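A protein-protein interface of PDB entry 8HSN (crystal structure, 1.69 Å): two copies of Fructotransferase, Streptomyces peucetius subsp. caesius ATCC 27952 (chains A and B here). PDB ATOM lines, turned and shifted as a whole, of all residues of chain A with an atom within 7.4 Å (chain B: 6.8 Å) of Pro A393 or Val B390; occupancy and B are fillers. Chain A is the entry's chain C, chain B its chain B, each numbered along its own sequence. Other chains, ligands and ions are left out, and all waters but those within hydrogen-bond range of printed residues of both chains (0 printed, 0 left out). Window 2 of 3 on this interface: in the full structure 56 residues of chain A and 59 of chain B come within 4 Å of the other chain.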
ATOM      1  N   HIS A 373     -12.891  19.878  13.555  1.00  0.00           N
ATOM      2  CA  HIS A 373     -13.017  20.663  12.335  1.00  0.00           C
ATOM      3  C   HIS A 373     -11.702  21.388  12.054  1.00  0.00           C
ATOM      4  O   HIS A 373     -11.673  22.570  11.690  1.00  0.00           O
ATOM      5  CB  HIS A 373     -14.178  21.661  12.413  1.00  0.00           C
ATOM      6  CG  HIS A 373     -15.529  21.021  12.531  1.00  0.00           C
ATOM      7  ND1 HIS A 373     -16.620  21.706  13.022  1.00  0.00           N
ATOM      8  CD2 HIS A 373     -15.968  19.779  12.225  1.00  0.00           C
ATOM      9  CE1 HIS A 373     -17.678  20.912  13.002  1.00  0.00           C
ATOM     10  NE2 HIS A 373     -17.308  19.733  12.531  1.00  0.00           N
ATOM     11  N   ALA A 375      -8.985  19.278  10.625  1.00  0.00           N
ATOM     12  CA  ALA A 375      -8.290  18.304   9.795  1.00  0.00           C
ATOM     13  C   ALA A 375      -9.357  17.381   9.233  1.00  0.00           C
ATOM     14  O   ALA A 375     -10.203  16.904   9.996  1.00  0.00           O
ATOM     15  CB  ALA A 375      -7.270  17.498  10.605  1.00  0.00           C
ATOM     16  N   THR A 376      -9.316  17.077   7.948  1.00  0.00           N
ATOM     17  CA  THR A 376     -10.049  15.933   7.436  1.00  0.00           C
ATOM     18  C   THR A 376      -9.413  14.650   7.972  1.00  0.00           C
ATOM     19  O   THR A 376      -8.309  14.657   8.536  1.00  0.00           O
ATOM     20  CB  THR A 376     -10.027  15.905   5.911  1.00  0.00           C
ATOM     21  OG1 THR A 376      -8.664  15.710   5.499  1.00  0.00           O
ATOM     22  CG2 THR A 376     -10.583  17.182   5.310  1.00  0.00           C
ATOM     23  N   THR A 377     -10.112  13.525   7.783  1.00  0.00           N
ATOM     24  CA  THR A 377      -9.528  12.240   8.152  1.00  0.00           C
ATOM     25  C   THR A 377      -8.165  12.057   7.495  1.00  0.00           C
ATOM     26  O   THR A 377      -7.210  11.605   8.139  1.00  0.00           O
ATOM     27  CB  THR A 377     -10.481  11.110   7.777  1.00  0.00           C
ATOM     28  OG1 THR A 377     -11.694  11.294   8.512  1.00  0.00           O
ATOM     29  CG2 THR A 377      -9.894   9.763   8.154  1.00  0.00           C
ATOM     30  N   VAL A 390     -13.065  15.031  15.647  1.00  0.00           N
ATOM     31  CA  VAL A 390     -14.296  15.359  14.937  1.00  0.00           C
ATOM     32  C   VAL A 390     -13.838  15.890  13.590  1.00  0.00           C
ATOM     33  O   VAL A 390     -13.370  17.027  13.492  1.00  0.00           O
ATOM     34  CB  VAL A 390     -15.158  16.381  15.675  1.00  0.00           C
ATOM     35  CG1 VAL A 390     -16.387  16.743  14.828  1.00  0.00           C
ATOM     36  CG2 VAL A 390     -15.554  15.826  17.027  1.00  0.00           C
ATOM     37  N   ALA A 391     -13.949  15.072  12.551  1.00  0.00           N
ATOM     38  CA  ALA A 391     -13.263  15.398  11.314  1.00  0.00           C
ATOM     39  C   ALA A 391     -13.909  16.561  10.579  1.00  0.00           C
ATOM     40  O   ALA A 391     -15.134  16.709  10.551  1.00  0.00           O
ATOM     41  CB  ALA A 391     -13.240  14.190  10.385  1.00  0.00           C
ATOM     42  N   THR A 392     -13.066  17.377   9.954  1.00  0.00           N
ATOM     43  CA  THR A 392     -13.526  18.219   8.854  1.00  0.00           C
ATOM     44  C   THR A 392     -14.077  17.320   7.763  1.00  0.00           C
ATOM     45  O   THR A 392     -13.407  16.353   7.382  1.00  0.00           O
ATOM     46  CB  THR A 392     -12.370  19.054   8.319  1.00  0.00           C
ATOM     47  OG1 THR A 392     -11.838  19.798   9.424  1.00  0.00           O
ATOM     48  CG2 THR A 392     -12.861  19.987   7.232  1.00  0.00           C
ATOM     49  N   PRO A 393     -15.302  17.548   7.291  1.00  0.00           N
ATOM     50  CA  PRO A 393     -15.890  16.598   6.326  1.00  0.00           C
ATOM     51  C   PRO A 393     -15.100  16.536   5.032  1.00  0.00           C
ATOM     52  O   PRO A 393     -14.511  17.521   4.580  1.00  0.00           O
ATOM     53  CB  PRO A 393     -17.315  17.118   6.107  1.00  0.00           C
ATOM     54  CG  PRO A 393     -17.460  18.323   6.920  1.00  0.00           C
ATOM     55  CD  PRO A 393     -16.314  18.447   7.867  1.00  0.00           C
ATOM     56  N   SER A 394     -15.038  15.327   4.468  1.00  0.00           N
ATOM     57  CA  SER A 394     -14.391  15.118   3.185  1.00  0.00           C
ATOM     58  C   SER A 394     -15.109  14.101   2.311  1.00  0.00           C
ATOM     59  O   SER A 394     -14.766  13.986   1.127  1.00  0.00           O
ATOM     60  CB  SER A 394     -12.934  14.670   3.368  1.00  0.00           C
ATOM     61  OG  SER A 394     -12.861  13.471   4.110  1.00  0.00           O
ATOM     62  N   HIS A 395     -16.066  13.360   2.832  1.00  0.00           N
ATOM     63  CA  HIS A 395     -16.814  12.438   1.986  1.00  0.00           C
ATOM     64  C   HIS A 395     -18.298  12.779   2.006  1.00  0.00           C
ATOM     65  O   HIS A 395     -18.864  13.088   3.059  1.00  0.00           O
ATOM     66  CB  HIS A 395     -16.577  10.984   2.411  1.00  0.00           C
ATOM     67  CG  HIS A 395     -15.124  10.619   2.511  1.00  0.00           C
ATOM     68  ND1 HIS A 395     -14.485  10.417   3.717  1.00  0.00           N
ATOM     69  CD2 HIS A 395     -14.182  10.448   1.552  1.00  0.00           C
ATOM     70  CE1 HIS A 395     -13.216  10.116   3.496  1.00  0.00           C
ATOM     71  NE2 HIS A 395     -13.008  10.130   2.191  1.00  0.00           N
ATOM     72  N   HIS A 396     -18.918  12.745   0.830  1.00  0.00           N
ATOM     73  CA  HIS A 396     -20.342  13.042   0.719  1.00  0.00           C
ATOM     74  C   HIS A 396     -21.148  11.820   1.159  1.00  0.00           C
ATOM     75  O   HIS A 396     -22.273  11.941   1.642  1.00  0.00           O
ATOM     76  CB  HIS A 396     -20.714  13.437  -0.713  1.00  0.00           C
ATOM     77  CG  HIS A 396     -20.043  14.689  -1.193  1.00  0.00           C
ATOM     78  ND1 HIS A 396     -20.433  15.950  -0.786  1.00  0.00           N
ATOM     79  CD2 HIS A 396     -19.017  14.872  -2.060  1.00  0.00           C
ATOM     80  CE1 HIS A 396     -19.669  16.853  -1.376  1.00  0.00           C
ATOM     81  NE2 HIS A 396     -18.801  16.226  -2.152  1.00  0.00           N
ATOM     82  N   ARG B 370     -16.972  24.227   2.567  1.00  0.00           N
ATOM     83  CA  ARG B 370     -17.293  23.692   3.880  1.00  0.00           C
ATOM     84  C   ARG B 370     -17.984  24.775   4.684  1.00  0.00           C
ATOM     85  O   ARG B 370     -17.528  25.921   4.707  1.00  0.00           O
ATOM     86  CB  ARG B 370     -16.034  23.192   4.585  1.00  0.00           C
ATOM     87  CG  ARG B 370     -15.613  21.864   4.007  1.00  0.00           C
ATOM     88  CD  ARG B 370     -14.278  21.413   4.460  1.00  0.00           C
ATOM     89  NE  ARG B 370     -13.966  20.120   3.859  1.00  0.00           N
ATOM     90  CZ  ARG B 370     -13.374  19.955   2.684  1.00  0.00           C
ATOM     91  NH1 ARG B 370     -13.015  20.990   1.938  1.00  0.00           N
ATOM     92  NH2 ARG B 370     -13.101  18.729   2.266  1.00  0.00           N
ATOM     93  N   VAL B 371     -19.116  24.424   5.280  1.00  0.00           N
ATOM     94  CA  VAL B 371     -19.916  25.339   6.083  1.00  0.00           C
ATOM     95  C   VAL B 371     -20.165  24.586   7.385  1.00  0.00           C
ATOM     96  O   VAL B 371     -21.001  23.675   7.426  1.00  0.00           O
ATOM     97  CB  VAL B 371     -21.224  25.733   5.398  1.00  0.00           C
ATOM     98  CG1 VAL B 371     -21.923  26.853   6.160  1.00  0.00           C
ATOM     99  CG2 VAL B 371     -20.967  26.214   3.961  1.00  0.00           C
ATOM    100  N   LEU B 372     -19.435  24.952   8.444  1.00  0.00           N
ATOM    101  CA  LEU B 372     -19.317  24.165   9.671  1.00  0.00           C
ATOM    102  C   LEU B 372     -19.675  25.043  10.867  1.00  0.00           C
ATOM    103  O   LEU B 372     -18.895  25.914  11.272  1.00  0.00           O
ATOM    104  CB  LEU B 372     -17.894  23.613   9.814  1.00  0.00           C
ATOM    105  CG  LEU B 372     -17.235  23.039   8.557  1.00  0.00           C
ATOM    106  CD1 LEU B 372     -15.821  22.607   8.870  1.00  0.00           C
ATOM    107  CD2 LEU B 372     -18.040  21.863   7.984  1.00  0.00           C
ATOM    108  N   HIS B 373     -20.859  24.830  11.441  1.00  0.00           N
ATOM    109  CA  HIS B 373     -21.315  25.668  12.549  1.00  0.00           C
ATOM    110  C   HIS B 373     -21.226  27.144  12.154  1.00  0.00           C
ATOM    111  O   HIS B 373     -20.844  28.008  12.946  1.00  0.00           O
ATOM    112  CB  HIS B 373     -20.520  25.399  13.831  1.00  0.00           C
ATOM    113  CG  HIS B 373     -20.718  24.031  14.417  1.00  0.00           C
ATOM    114  ND1 HIS B 373     -19.860  23.502  15.357  1.00  0.00           N
ATOM    115  CD2 HIS B 373     -21.662  23.080  14.189  1.00  0.00           C
ATOM    116  CE1 HIS B 373     -20.279  22.293  15.697  1.00  0.00           C
ATOM    117  NE2 HIS B 373     -21.365  22.011  15.000  1.00  0.00           N
ATOM    118  N   SER B 374     -21.602  27.428  10.910  1.00  0.00           N
ATOM    119  CA  SER B 374     -21.560  28.768  10.343  1.00  0.00           C
ATOM    120  C   SER B 374     -22.859  29.114   9.632  1.00  0.00           C
ATOM    121  O   SER B 374     -22.884  30.016   8.789  1.00  0.00           O
ATOM    122  CB  SER B 374     -20.369  28.881   9.386  1.00  0.00           C
ATOM    123  OG  SER B 374     -20.241  30.194   8.889  1.00  0.00           O
ATOM    124  N   ALA B 375     -23.903  28.328   9.855  1.00  0.00           N
ATOM    125  CA  ALA B 375     -25.209  28.533   9.257  1.00  0.00           C
ATOM    126  C   ALA B 375     -26.113  27.437   9.780  1.00  0.00           C
ATOM    127  O   ALA B 375     -25.711  26.272   9.730  1.00  0.00           O
ATOM    128  CB  ALA B 375     -25.163  28.460   7.744  1.00  0.00           C
ATOM    129  N   PHE B 388     -20.040  20.714   1.730  1.00  0.00           N
ATOM    130  CA  PHE B 388     -20.117  19.956   2.966  1.00  0.00           C
ATOM    131  C   PHE B 388     -20.739  20.843   4.028  1.00  0.00           C
ATOM    132  O   PHE B 388     -20.228  21.932   4.305  1.00  0.00           O
ATOM    133  CB  PHE B 388     -18.736  19.483   3.434  1.00  0.00           C
ATOM    134  CG  PHE B 388     -17.996  18.650   2.430  1.00  0.00           C
ATOM    135  CD1 PHE B 388     -18.183  17.279   2.375  1.00  0.00           C
ATOM    136  CD2 PHE B 388     -17.108  19.234   1.547  1.00  0.00           C
ATOM    137  CE1 PHE B 388     -17.486  16.508   1.461  1.00  0.00           C
ATOM    138  CE2 PHE B 388     -16.411  18.461   0.635  1.00  0.00           C
ATOM    139  CZ  PHE B 388     -16.608  17.098   0.593  1.00  0.00           C
ATOM    140  N   MET B 389     -21.830  20.372   4.617  1.00  0.00           N
ATOM    141  CA  MET B 389     -22.548  21.084   5.665  1.00  0.00           C
ATOM    142  C   MET B 389     -22.565  20.319   6.970  1.00  0.00           C
ATOM    143  O   MET B 389     -22.958  19.148   7.013  1.00  0.00           O
ATOM    144  CB  MET B 389     -23.975  21.400   5.204  1.00  0.00           C
ATOM    145  CG  MET B 389     -24.930  21.966   6.249  1.00  0.00           C
ATOM    146  SD  MET B 389     -24.527  23.604   6.746  1.00  0.00           S
ATOM    147  CE  MET B 389     -26.077  24.262   7.313  1.00  0.00           C
ATOM    148  N   VAL B 390     -22.109  20.987   8.021  1.00  0.00           N
ATOM    149  CA  VAL B 390     -22.317  20.578   9.402  1.00  0.00           C
ATOM    150  C   VAL B 390     -23.098  21.725  10.030  1.00  0.00           C
ATOM    151  O   VAL B 390     -22.528  22.772  10.371  1.00  0.00           O
ATOM    152  CB  VAL B 390     -21.010  20.310  10.156  1.00  0.00           C
ATOM    153  CG1 VAL B 390     -21.287  19.976  11.619  1.00  0.00           C
ATOM    154  CG2 VAL B 390     -20.255  19.178   9.494  1.00  0.00           C
ATOM    155  N   ALA B 391     -24.414  21.566  10.140  1.00  0.00           N
ATOM    156  CA  ALA B 391     -25.270  22.706  10.436  1.00  0.00           C
ATOM    157  C   ALA B 391     -25.040  23.243  11.840  1.00  0.00           C
ATOM    158  O   ALA B 391     -24.855  22.483  12.801  1.00  0.00           O
ATOM    159  CB  ALA B 391     -26.751  22.317  10.310  1.00  0.00           C
ATOM    160  N   THR B 392     -25.128  24.556  11.975  1.00  0.00           N
ATOM    161  CA  THR B 392     -25.393  25.123  13.288  1.00  0.00           C
ATOM    162  C   THR B 392     -26.710  24.548  13.786  1.00  0.00           C
ATOM    163  O   THR B 392     -27.707  24.608  13.060  1.00  0.00           O
ATOM    164  CB  THR B 392     -25.480  26.634  13.202  1.00  0.00           C
ATOM    165  OG1 THR B 392     -24.267  27.116  12.603  1.00  0.00           O
ATOM    166  CG2 THR B 392     -25.683  27.238  14.598  1.00  0.00           C
ATOM    167  N   PRO B 393     -26.762  23.990  14.998  1.00  0.00           N
ATOM    168  CA  PRO B 393     -28.014  23.374  15.455  1.00  0.00           C
ATOM    169  C   PRO B 393     -29.184  24.342  15.404  1.00  0.00           C
ATOM    170  O   PRO B 393     -29.045  25.546  15.645  1.00  0.00           O
ATOM    171  CB  PRO B 393     -27.691  22.951  16.893  1.00  0.00           C
ATOM    172  CG  PRO B 393     -26.240  22.719  16.893  1.00  0.00           C
ATOM    173  CD  PRO B 393     -25.667  23.773  15.964  1.00  0.00           C
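The guanidinium group (NE) of Arg B370 sits at hydrogen-bond distance from the backbone carbonyl oxygen (O) of Pro A393.
Pro A393 touches just these residues of chain B: Arg B370 (2.8 Å), Leu B372 (3.7 Å), Phe B388 (3.8 Å) and Val B390 (3.9 Å). Printed residues of chain B within 4 Å of Ser A394: Arg B370 and Phe B388. Of the printed residues of chain A, Phe B388 touches Pro A393, Ser A394, His A395 and His A396. The nearest residue of chain B that does not touch Pro A393 is Met B389 (5.3 Å).
Of the 12 printed residues of chain B, 5 touch a printed residue of chain A. Hydrophobic or aromatic side chains of chain B that line the printed part of chain A: Leu B372, His B373, Phe B388 and Val B390. Along chain B the printed residues that touch a printed residue of chain A span positions 370 to 390. Of the 11 printed residues of chain A, 6 touch a printed residue of chain B. Printed residues of chain A that touch a printed residue of chain B: His A373, Thr A392, Pro A393, Ser A394, His A395 and His A396. Along chain A the printed residues that touch a printed residue of chain B span positions 373 to 396. Among the printed residues, 12 pairs touch across the chains. Among the printed residues, no Asp or Glu carboxylate lies within 4 Å of a Lys or Arg side-chain nitrogen of the other chain.
N of Thr A392 is in hydrogen-bond range of O of Ala A375, at 2.9 Å. The backbone NH (N) of Val B390 sits at hydrogen-bond distance from the backbone carbonyl oxygen (O) of Val B371. N of His A373 sits at hydrogen-bond distance from O of Val A390, 2.9 Å away. The side-chain hydroxyl of Ser A394 sits close to a ring nitrogen (ND1) of His A395, 3.5 Å away. The backbone NH of His B373 lies within hydrogen-bond range of the backbone carbonyl oxygen of Val B390 (2.9 Å). The backbone carbonyl oxygen (O) of Phe B388 is in hydrogen-bond range of the backbone NH (N) of Val B371 (2.9 Å).
His A373 touches its own counterpart, His B373. His A373 touches Val B390, but with the chains exchanged Val A390 does not touch His B373 (6.8 Å). Pro A393 touches Val B390, but with the chains exchanged Val A390 does not touch Pro B393 (11.7 Å).
Among the printed residues, merely in contact across the chains: His A373 with Leu B372 (3.9 Å), His A373 with His B373 (3.99 Å), His A373 with Val B390 (3.98 Å), Thr A392 with Arg B370 (3.4 Å), Pro A393 with Leu B372 (3.7 Å), Pro A393 with Phe B388 (3.8 Å), Pro A393 with Val B390 (3.9 Å), Ser A394 with Arg B370 (3.9 Å), Ser A394 with Phe B388 (3.5 Å), His A395 with Phe B388 (3.7 Å) and His A396 with Phe B388 (3.6 Å).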
